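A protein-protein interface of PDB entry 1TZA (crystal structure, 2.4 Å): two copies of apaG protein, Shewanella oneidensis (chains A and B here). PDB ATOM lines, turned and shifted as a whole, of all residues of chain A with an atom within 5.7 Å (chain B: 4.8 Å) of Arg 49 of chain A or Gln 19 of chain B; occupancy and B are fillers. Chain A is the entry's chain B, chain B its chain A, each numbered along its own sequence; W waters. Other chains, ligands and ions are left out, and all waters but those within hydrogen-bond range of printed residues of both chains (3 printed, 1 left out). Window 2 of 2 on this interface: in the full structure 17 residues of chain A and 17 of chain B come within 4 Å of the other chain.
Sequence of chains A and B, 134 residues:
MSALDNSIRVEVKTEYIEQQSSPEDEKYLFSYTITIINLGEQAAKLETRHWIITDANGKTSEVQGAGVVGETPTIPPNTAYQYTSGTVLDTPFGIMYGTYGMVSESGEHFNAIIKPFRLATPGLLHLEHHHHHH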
ATOM      1  N   LEU A  46      18.016  32.516  -4.573  1.00  0.00           N
ATOM      2  CA  LEU A  46      17.836  31.766  -5.803  1.00  0.00           C
ATOM      3  C   LEU A  46      16.351  31.894  -6.157  1.00  0.00           C
ATOM      4  O   LEU A  46      15.492  31.395  -5.439  1.00  0.00           O
ATOM      5  CB  LEU A  46      18.234  30.299  -5.599  1.00  0.00           C
ATOM      6  CG  LEU A  46      18.305  29.481  -6.893  1.00  0.00           C
ATOM      7  CD1 LEU A  46      19.160  28.255  -6.670  1.00  0.00           C
ATOM      8  CD2 LEU A  46      16.896  29.100  -7.358  1.00  0.00           C
ATOM      9  N   GLU A  47      16.053  32.571  -7.261  1.00  0.00           N
ATOM     10  CA  GLU A  47      14.672  32.777  -7.668  1.00  0.00           C
ATOM     11  C   GLU A  47      14.174  31.856  -8.772  1.00  0.00           C
ATOM     12  O   GLU A  47      13.000  31.473  -8.790  1.00  0.00           O
ATOM     13  CB  GLU A  47      14.474  34.228  -8.099  1.00  0.00           C
ATOM     14  CG  GLU A  47      14.437  35.220  -6.946  1.00  0.00           C
ATOM     15  CD  GLU A  47      14.212  36.651  -7.418  1.00  0.00           C
ATOM     16  OE1 GLU A  47      14.041  37.545  -6.560  1.00  0.00           O
ATOM     17  OE2 GLU A  47      14.211  36.880  -8.648  1.00  0.00           O
ATOM     18  N   THR A  48      15.058  31.513  -9.697  1.00  0.00           N
ATOM     19  CA  THR A  48      14.673  30.642 -10.796  1.00  0.00           C
ATOM     20  C   THR A  48      15.774  29.669 -11.158  1.00  0.00           C
ATOM     21  O   THR A  48      16.900  29.788 -10.683  1.00  0.00           O
ATOM     22  CB  THR A  48      14.337  31.444 -12.069  1.00  0.00           C
ATOM     23  OG1 THR A  48      15.472  32.235 -12.436  1.00  0.00           O
ATOM     24  CG2 THR A  48      13.142  32.346 -11.842  1.00  0.00           C
ATOM     25  N   ARG A  49      15.428  28.706 -12.007  1.00  0.00           N
ATOM     26  CA  ARG A  49      16.378  27.713 -12.487  1.00  0.00           C
ATOM     27  C   ARG A  49      16.147  27.536 -13.981  1.00  0.00           C
ATOM     28  O   ARG A  49      15.056  27.793 -14.488  1.00  0.00           O
ATOM     29  CB  ARG A  49      16.189  26.370 -11.773  1.00  0.00           C
ATOM     30  CG  ARG A  49      14.923  25.620 -12.150  1.00  0.00           C
ATOM     31  CD  ARG A  49      14.812  24.312 -11.359  1.00  0.00           C
ATOM     32  NE  ARG A  49      13.583  23.585 -11.665  1.00  0.00           N
ATOM     33  CZ  ARG A  49      12.364  24.025 -11.372  1.00  0.00           C
ATOM     34  NH1 ARG A  49      12.211  25.187 -10.755  1.00  0.00           N
ATOM     35  NH2 ARG A  49      11.297  23.309 -11.707  1.00  0.00           N
ATOM     36  N   HIS A  50      17.185  27.104 -14.681  1.00  0.00           N
ATOM     37  CA  HIS A  50      17.099  26.886 -16.115  1.00  0.00           C
ATOM     38  C   HIS A  50      18.030  25.746 -16.509  1.00  0.00           C
ATOM     39  O   HIS A  50      19.243  25.927 -16.682  1.00  0.00           O
ATOM     40  CB  HIS A  50      17.454  28.172 -16.875  1.00  0.00           C
ATOM     41  CG  HIS A  50      17.324  28.046 -18.360  1.00  0.00           C
ATOM     42  ND1 HIS A  50      16.614  27.030 -18.962  1.00  0.00           N
ATOM     43  CD2 HIS A  50      17.813  28.810 -19.366  1.00  0.00           C
ATOM     44  CE1 HIS A  50      16.672  27.170 -20.275  1.00  0.00           C
ATOM     45  NE2 HIS A  50      17.394  28.242 -20.546  1.00  0.00           N
ATOM     46  N   TRP A  51      17.437  24.567 -16.637  1.00  0.00           N
ATOM     47  CA  TRP A  51      18.151  23.360 -16.992  1.00  0.00           C
ATOM     48  C   TRP A  51      18.105  23.038 -18.479  1.00  0.00           C
ATOM     49  O   TRP A  51      17.123  23.305 -19.167  1.00  0.00           O
ATOM     50  CB  TRP A  51      17.567  22.172 -16.220  1.00  0.00           C
ATOM     51  CG  TRP A  51      17.902  22.162 -14.754  1.00  0.00           C
ATOM     52  CD1 TRP A  51      17.024  22.151 -13.711  1.00  0.00           C
ATOM     53  CD2 TRP A  51      19.209  22.140 -14.177  1.00  0.00           C
ATOM     54  NE1 TRP A  51      17.703  22.120 -12.517  1.00  0.00           N
ATOM     55  CE2 TRP A  51      19.046  22.110 -12.773  1.00  0.00           C
ATOM     56  CE3 TRP A  51      20.504  22.139 -14.712  1.00  0.00           C
ATOM     57  CZ2 TRP A  51      20.135  22.083 -11.892  1.00  0.00           C
ATOM     58  CZ3 TRP A  51      21.592  22.112 -13.832  1.00  0.00           C
ATOM     59  CH2 TRP A  51      21.397  22.083 -12.438  1.00  0.00           C
ATOM     60  N   VAL A  63      14.068  22.888 -18.745  1.00  0.00           N
ATOM     61  CA  VAL A  63      13.178  23.102 -17.626  1.00  0.00           C
ATOM     62  C   VAL A  63      13.502  24.474 -17.053  1.00  0.00           C
ATOM     63  O   VAL A  63      14.648  24.753 -16.675  1.00  0.00           O
ATOM     64  CB  VAL A  63      13.376  22.029 -16.514  1.00  0.00           C
ATOM     65  CG1 VAL A  63      12.300  22.180 -15.451  1.00  0.00           C
ATOM     66  CG2 VAL A  63      13.347  20.621 -17.112  1.00  0.00           C
ATOM     67  N   GLN A  64      12.491  25.335 -17.028  1.00  0.00           N
ATOM     68  CA  GLN A  64      12.607  26.683 -16.490  1.00  0.00           C
ATOM     69  C   GLN A  64      11.529  26.762 -15.410  1.00  0.00           C
ATOM     70  O   GLN A  64      10.375  26.405 -15.657  1.00  0.00           O
ATOM     71  CB  GLN A  64      12.333  27.712 -17.591  1.00  0.00           C
ATOM     72  CG  GLN A  64      13.569  28.395 -18.171  1.00  0.00           C
ATOM     73  CD  GLN A  64      14.048  29.570 -17.323  1.00  0.00           C
ATOM     74  OE1 GLN A  64      14.968  30.297 -17.710  1.00  0.00           O
ATOM     75  NE2 GLN A  64      13.424  29.760 -16.162  1.00  0.00           N
ATOM     76  N   GLY A  65      11.895  27.208 -14.215  1.00  0.00           N
ATOM     77  CA  GLY A  65      10.908  27.287 -13.151  1.00  0.00           C
ATOM     78  C   GLY A  65      11.324  28.146 -11.979  1.00  0.00           C
ATOM     79  O   GLY A  65      12.445  28.648 -11.934  1.00  0.00           O
ATOM     80  N   ALA A  66      10.415  28.320 -11.027  1.00  0.00           N
ATOM     81  CA  ALA A  66      10.691  29.128  -9.844  1.00  0.00           C
ATOM     82  C   ALA A  66      11.393  28.292  -8.783  1.00  0.00           C
ATOM     83  O   ALA A  66      10.959  27.181  -8.471  1.00  0.00           O
ATOM     84  CB  ALA A  66       9.386  29.704  -9.276  1.00  0.00           C
ATOM     85  N   GLY A  67      12.481  28.832  -8.243  1.00  0.00           N
ATOM     86  CA  GLY A  67      13.231  28.146  -7.205  1.00  0.00           C
ATOM     87  C   GLY A  67      13.698  26.760  -7.589  1.00  0.00           C
ATOM     88  O   GLY A  67      13.727  26.418  -8.766  1.00  0.00           O
ATOM     89  N   VAL A  68      14.088  25.980  -6.586  1.00  0.00           N
ATOM     90  CA  VAL A  68      14.542  24.611  -6.769  1.00  0.00           C
ATOM     91  C   VAL A  68      13.793  23.777  -5.738  1.00  0.00           C
ATOM     92  O   VAL A  68      13.645  24.191  -4.588  1.00  0.00           O
ATOM     93  CB  VAL A  68      16.069  24.463  -6.530  1.00  0.00           C
ATOM     94  CG1 VAL A  68      16.830  24.992  -7.723  1.00  0.00           C
ATOM     95  CG2 VAL A  68      16.480  25.215  -5.272  1.00  0.00           C
ATOM     96  N   VAL A  69      13.337  22.601  -6.153  1.00  0.00           N
ATOM     97  CA  VAL A  69      12.559  21.722  -5.296  1.00  0.00           C
ATOM     98  C   VAL A  69      11.488  22.478  -4.501  1.00  0.00           C
ATOM     99  O   VAL A  69      11.253  22.196  -3.329  1.00  0.00           O
ATOM    100  CB  VAL A  69      13.455  20.877  -4.342  1.00  0.00           C
ATOM    101  CG1 VAL A  69      14.222  19.845  -5.161  1.00  0.00           C
ATOM    102  CG2 VAL A  69      14.422  21.759  -3.568  1.00  0.00           C
ATOM    103  N   TYR A  83      20.697  20.699  -1.950  1.00  0.00           N
ATOM    104  CA  TYR A  83      19.407  20.105  -2.261  1.00  0.00           C
ATOM    105  C   TYR A  83      19.547  18.955  -3.251  1.00  0.00           C
ATOM    106  O   TYR A  83      20.570  18.817  -3.934  1.00  0.00           O
ATOM    107  CB  TYR A  83      18.460  21.171  -2.809  1.00  0.00           C
ATOM    108  CG  TYR A  83      18.580  21.444  -4.287  1.00  0.00           C
ATOM    109  CD1 TYR A  83      17.859  20.685  -5.213  1.00  0.00           C
ATOM    110  CD2 TYR A  83      19.385  22.482  -4.766  1.00  0.00           C
ATOM    111  CE1 TYR A  83      17.932  20.957  -6.586  1.00  0.00           C
ATOM    112  CE2 TYR A  83      19.464  22.759  -6.138  1.00  0.00           C
ATOM    113  CZ  TYR A  83      18.733  21.994  -7.039  1.00  0.00           C
ATOM    114  OH  TYR A  83      18.779  22.264  -8.384  1.00  0.00           O
ATOM    115  N   THR A  99      21.572  27.248 -15.575  1.00  0.00           N
ATOM    116  CA  THR A  99      21.807  28.456 -14.791  1.00  0.00           C
ATOM    117  C   THR A  99      20.710  28.699 -13.764  1.00  0.00           C
ATOM    118  O   THR A  99      19.574  28.265 -13.944  1.00  0.00           O
ATOM    119  CB  THR A  99      21.863  29.711 -15.692  1.00  0.00           C
ATOM    120  OG1 THR A  99      20.703  29.737 -16.530  1.00  0.00           O
ATOM    121  CG2 THR A  99      23.115  29.708 -16.568  1.00  0.00           C
ATOM    122  N   TYR A 100      21.069  29.392 -12.686  1.00  0.00           N
ATOM    123  CA  TYR A 100      20.126  29.765 -11.634  1.00  0.00           C
ATOM    124  C   TYR A 100      19.956  31.278 -11.715  1.00  0.00           C
ATOM    125  O   TYR A 100      20.923  32.002 -11.975  1.00  0.00           O
ATOM    126  CB  TYR A 100      20.669  29.430 -10.243  1.00  0.00           C
ATOM    127  CG  TYR A 100      20.737  27.959  -9.906  1.00  0.00           C
ATOM    128  CD1 TYR A 100      19.654  27.114 -10.146  1.00  0.00           C
ATOM    129  CD2 TYR A 100      21.871  27.421  -9.303  1.00  0.00           C
ATOM    130  CE1 TYR A 100      19.700  25.769  -9.793  1.00  0.00           C
ATOM    131  CE2 TYR A 100      21.926  26.080  -8.941  1.00  0.00           C
ATOM    132  CZ  TYR A 100      20.840  25.261  -9.191  1.00  0.00           C
ATOM    133  OH  TYR A 100      20.905  23.934  -8.849  1.00  0.00           O
ATOM    134  N   GLY A 101      18.734  31.753 -11.494  1.00  0.00           N
ATOM    135  CA  GLY A 101      18.478  33.185 -11.522  1.00  0.00           C
ATOM    136  C   GLY A 101      18.605  33.706 -10.104  1.00  0.00           C
ATOM    137  O   GLY A 101      17.732  33.472  -9.275  1.00  0.00           O
ATOM    138  N   TYR B  16       6.616  14.837  -3.245  1.00  0.00           N
ATOM    139  CA  TYR B  16       6.691  15.550  -4.506  1.00  0.00           C
ATOM    140  C   TYR B  16       8.031  16.248  -4.489  1.00  0.00           C
ATOM    141  O   TYR B  16       8.292  17.085  -3.623  1.00  0.00           O
ATOM    142  CB  TYR B  16       5.572  16.581  -4.631  1.00  0.00           C
ATOM    143  CG  TYR B  16       5.727  17.486  -5.832  1.00  0.00           C
ATOM    144  CD1 TYR B  16       5.915  16.958  -7.106  1.00  0.00           C
ATOM    145  CD2 TYR B  16       5.675  18.873  -5.696  1.00  0.00           C
ATOM    146  CE1 TYR B  16       6.050  17.787  -8.223  1.00  0.00           C
ATOM    147  CE2 TYR B  16       5.806  19.716  -6.807  1.00  0.00           C
ATOM    148  CZ  TYR B  16       5.995  19.162  -8.068  1.00  0.00           C
ATOM    149  OH  TYR B  16       6.140  19.977  -9.166  1.00  0.00           O
ATOM    150  N   ILE B  17       8.888  15.907  -5.436  1.00  0.00           N
ATOM    151  CA  ILE B  17      10.198  16.517  -5.466  1.00  0.00           C
ATOM    152  C   ILE B  17      10.265  17.832  -6.230  1.00  0.00           C
ATOM    153  O   ILE B  17      10.488  18.883  -5.637  1.00  0.00           O
ATOM    154  CB  ILE B  17      11.236  15.534  -6.032  1.00  0.00           C
ATOM    155  CG1 ILE B  17      11.169  14.223  -5.242  1.00  0.00           C
ATOM    156  CG2 ILE B  17      12.627  16.135  -5.942  1.00  0.00           C
ATOM    157  CD1 ILE B  17      11.319  14.404  -3.723  1.00  0.00           C
ATOM    158  N   GLU B  18      10.037  17.789  -7.537  1.00  0.00           N
ATOM    159  CA  GLU B  18      10.156  19.007  -8.321  1.00  0.00           C
ATOM    160  C   GLU B  18       9.426  18.921  -9.647  1.00  0.00           C
ATOM    161  O   GLU B  18       9.209  17.831 -10.182  1.00  0.00           O
ATOM    162  CB  GLU B  18      11.645  19.264  -8.557  1.00  0.00           C
ATOM    163  CG  GLU B  18      12.016  20.555  -9.259  1.00  0.00           C
ATOM    164  CD  GLU B  18      13.515  20.665  -9.453  1.00  0.00           C
ATOM    165  OE1 GLU B  18      14.086  19.834 -10.196  1.00  0.00           O
ATOM    166  OE2 GLU B  18      14.127  21.569  -8.854  1.00  0.00           O
ATOM    167  N   GLN B  19       9.040  20.077 -10.171  1.00  0.00           N
ATOM    168  CA  GLN B  19       8.361  20.140 -11.458  1.00  0.00           C
ATOM    169  C   GLN B  19       9.436  20.036 -12.548  1.00  0.00           C
ATOM    170  O   GLN B  19      10.488  20.667 -12.449  1.00  0.00           O
ATOM    171  CB  GLN B  19       7.620  21.471 -11.586  1.00  0.00           C
ATOM    172  CG  GLN B  19       6.475  21.475 -12.589  1.00  0.00           C
ATOM    173  CD  GLN B  19       5.737  22.805 -12.626  1.00  0.00           C
ATOM    174  OE1 GLN B  19       6.219  23.785 -13.199  1.00  0.00           O
ATOM    175  NE2 GLN B  19       4.567  22.847 -12.000  1.00  0.00           N
ATOM    176  N   GLN B  20       9.182  19.236 -13.578  1.00  0.00           N
ATOM    177  CA  GLN B  20      10.147  19.090 -14.663  1.00  0.00           C
ATOM    178  C   GLN B  20       9.504  19.489 -15.980  1.00  0.00           C
ATOM    179  O   GLN B  20       9.966  19.089 -17.048  1.00  0.00           O
ATOM    180  CB  GLN B  20      10.632  17.641 -14.764  1.00  0.00           C
ATOM    181  CG  GLN B  20      11.188  17.101 -13.472  1.00  0.00           C
ATOM    182  CD  GLN B  20      12.269  17.988 -12.901  1.00  0.00           C
ATOM    183  OE1 GLN B  20      12.498  18.007 -11.690  1.00  0.00           O
ATOM    184  NE2 GLN B  20      12.943  18.732 -13.771  1.00  0.00           N
ATOM    185  N   SER B  21       8.452  20.296 -15.900  1.00  0.00           N
ATOM    186  CA  SER B  21       7.717  20.721 -17.087  1.00  0.00           C
ATOM    187  C   SER B  21       8.412  21.622 -18.117  1.00  0.00           C
ATOM    188  O   SER B  21       9.180  22.520 -17.776  1.00  0.00           O
ATOM    189  CB  SER B  21       6.407  21.399 -16.672  1.00  0.00           C
ATOM    190  OG  SER B  21       5.493  20.472 -16.136  1.00  0.00           O
ATOM    191  N   LYS B  27       5.356  17.806 -16.390  1.00  0.00           N
ATOM    192  CA  LYS B  27       6.090  16.692 -15.798  1.00  0.00           C
ATOM    193  C   LYS B  27       6.261  16.973 -14.312  1.00  0.00           C
ATOM    194  O   LYS B  27       6.624  18.081 -13.917  1.00  0.00           O
ATOM    195  CB  LYS B  27       7.475  16.536 -16.440  1.00  0.00           C
ATOM    196  CG  LYS B  27       7.475  16.148 -17.908  1.00  0.00           C
ATOM    197  CD  LYS B  27       8.895  16.245 -18.478  1.00  0.00           C
ATOM    198  CE  LYS B  27       8.913  16.163 -20.004  1.00  0.00           C
ATOM    199  NZ  LYS B  27       8.502  14.826 -20.522  1.00  0.00           N
ATOM    200  N   TYR B  28       6.002  15.965 -13.489  1.00  0.00           N
ATOM    201  CA  TYR B  28       6.130  16.121 -12.051  1.00  0.00           C
ATOM    202  C   TYR B  28       6.944  14.968 -11.478  1.00  0.00           C
ATOM    203  O   TYR B  28       6.552  13.806 -11.598  1.00  0.00           O
ATOM    204  CB  TYR B  28       4.742  16.176 -11.411  1.00  0.00           C
ATOM    205  CG  TYR B  28       3.859  17.235 -12.020  1.00  0.00           C
ATOM    206  CD1 TYR B  28       3.090  16.967 -13.153  1.00  0.00           C
ATOM    207  CD2 TYR B  28       3.817  18.518 -11.485  1.00  0.00           C
ATOM    208  CE1 TYR B  28       2.299  17.960 -13.742  1.00  0.00           C
ATOM    209  CE2 TYR B  28       3.033  19.516 -12.064  1.00  0.00           C
ATOM    210  CZ  TYR B  28       2.278  19.229 -13.190  1.00  0.00           C
ATOM    211  OH  TYR B  28       1.519  20.218 -13.767  1.00  0.00           O
HETATM  212  O   HOH W   1       8.769  21.243  -5.553  1.00  0.00           O
HETATM  213  O   HOH W   2      16.716  21.546  -9.959  1.00  0.00           O
HETATM  214  O   HOH W   3      14.098  21.148 -12.691  1.00  0.00           O
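The side-chain carboxylate (OE2) of Glu 18 of chain B lies within salt-bridge range of the guanidinium group (NE) of Arg 49 of chain A.
The backbone carbonyl oxygen (O) of Gln 19 of chain B sits at hydrogen-bond distance from the guanidinium group (NH2) of Arg 49 of chain A (2.9 Å).
OE2 of Glu 18 of chain B is in hydrogen-bond range of N of Val 69 of chain A (3.0 Å).
OH of Tyr 16 of chain B lies within hydrogen-bond range of N of Gln 19 of chain B (3.1 Å).
OE1 of Glu 18 of chain B lies close to OE1 of Gln 20 of chain B.
The backbone carbonyl oxygen (O) of Arg 49 of chain A is in hydrogen-bond range of the side-chain amide nitrogen (NE2) of Gln 64 of chain A, at 3.1 Å.
The side-chain hydroxyl (OG) of Ser 21 of chain B lies within hydrogen-bond range of the backbone NH (N) of Lys 27 of chain B.
The backbone NH (N) of Arg 49 of chain A is in hydrogen-bond range of the backbone carbonyl oxygen (O) of Gly 65 of chain A (3.0 Å).
The backbone carbonyl oxygen of Val 63 of chain A sits at hydrogen-bond distance from the backbone NH of Trp 51 of chain A (2.8 Å).
O of Gln 19 of chain B touches CG1 of Val 63 of chain A, at 3.8 Å.
O of Gln 20 of chain B touches CG2 of Val 63 of chain A, at 3.7 Å.
Ser 21 of chain B touches Val 63 of chain A (O to CG1, 3.9 Å).
Val 68 of chain A touches Glu 18 of chain B.
Val 69 of chain A touches Ile 17 of chain B.
Trp 51 of chain A touches none of the printed residues of chain B.
Of the printed residues of chain B, Val 68 of chain A touches Glu 18.
Of the printed residues of chain B, Val 69 of chain A touches Ile 17 and Glu 18.
Printed residues of chain A within 4 Å of Ile 17 of chain B: Val 69 (3.5 Å).
Printed residues of chain A within 4 Å of Gln 19 of chain B: Arg 49 and Val 63.
Of the printed residues of chain A, Gln 20 of chain B touches Val 63 (3.7 Å).
Printed residues of chain A within 4 Å of Ser 21 of chain B: Val 63.
Of the 17 printed residues of chain A, 4 touch a printed residue of chain B.
Hydrophobic or aromatic side chains of chain A that line the printed part of chain B: Val 63 and Val 69.
Printed residues of chain B that touch a printed residue of chain A: Ile 17, Glu 18, Gln 19, Gln 20 and Ser 21.
Among the printed residues, Asp or Glu carboxylates within 4 Å of a Lys or Arg side-chain nitrogen of the other chain: Arg 49 of chain A with Glu 18 of chain B.
No position is printed for both chains.
Of the 8 pairs that touch across the chains among the printed residues, none has its exchanged pair printed and touching as well.
Water W2 lies within hydrogen-bond range of OH of Tyr 83 of chain A (2.7 Å), NE1 of Trp 51 of chain A (2.8 Å) and OE2 of Glu 18 of chain B (2.8 Å).
Water W3 lies within hydrogen-bond range of the guanidinium group (NE) of Arg 49 of chain A (2.7 Å), the side-chain carboxylate (OE1) of Glu 18 of chain B (2.8 Å) and the side-chain amide nitrogen (NE2) of Gln 20 of chain B (2.9 Å).
Water W1 lies within hydrogen-bond range of the backbone carbonyl oxygen of Ile 17 of chain B and the backbone carbonyl oxygen of Val 69 of chain A.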
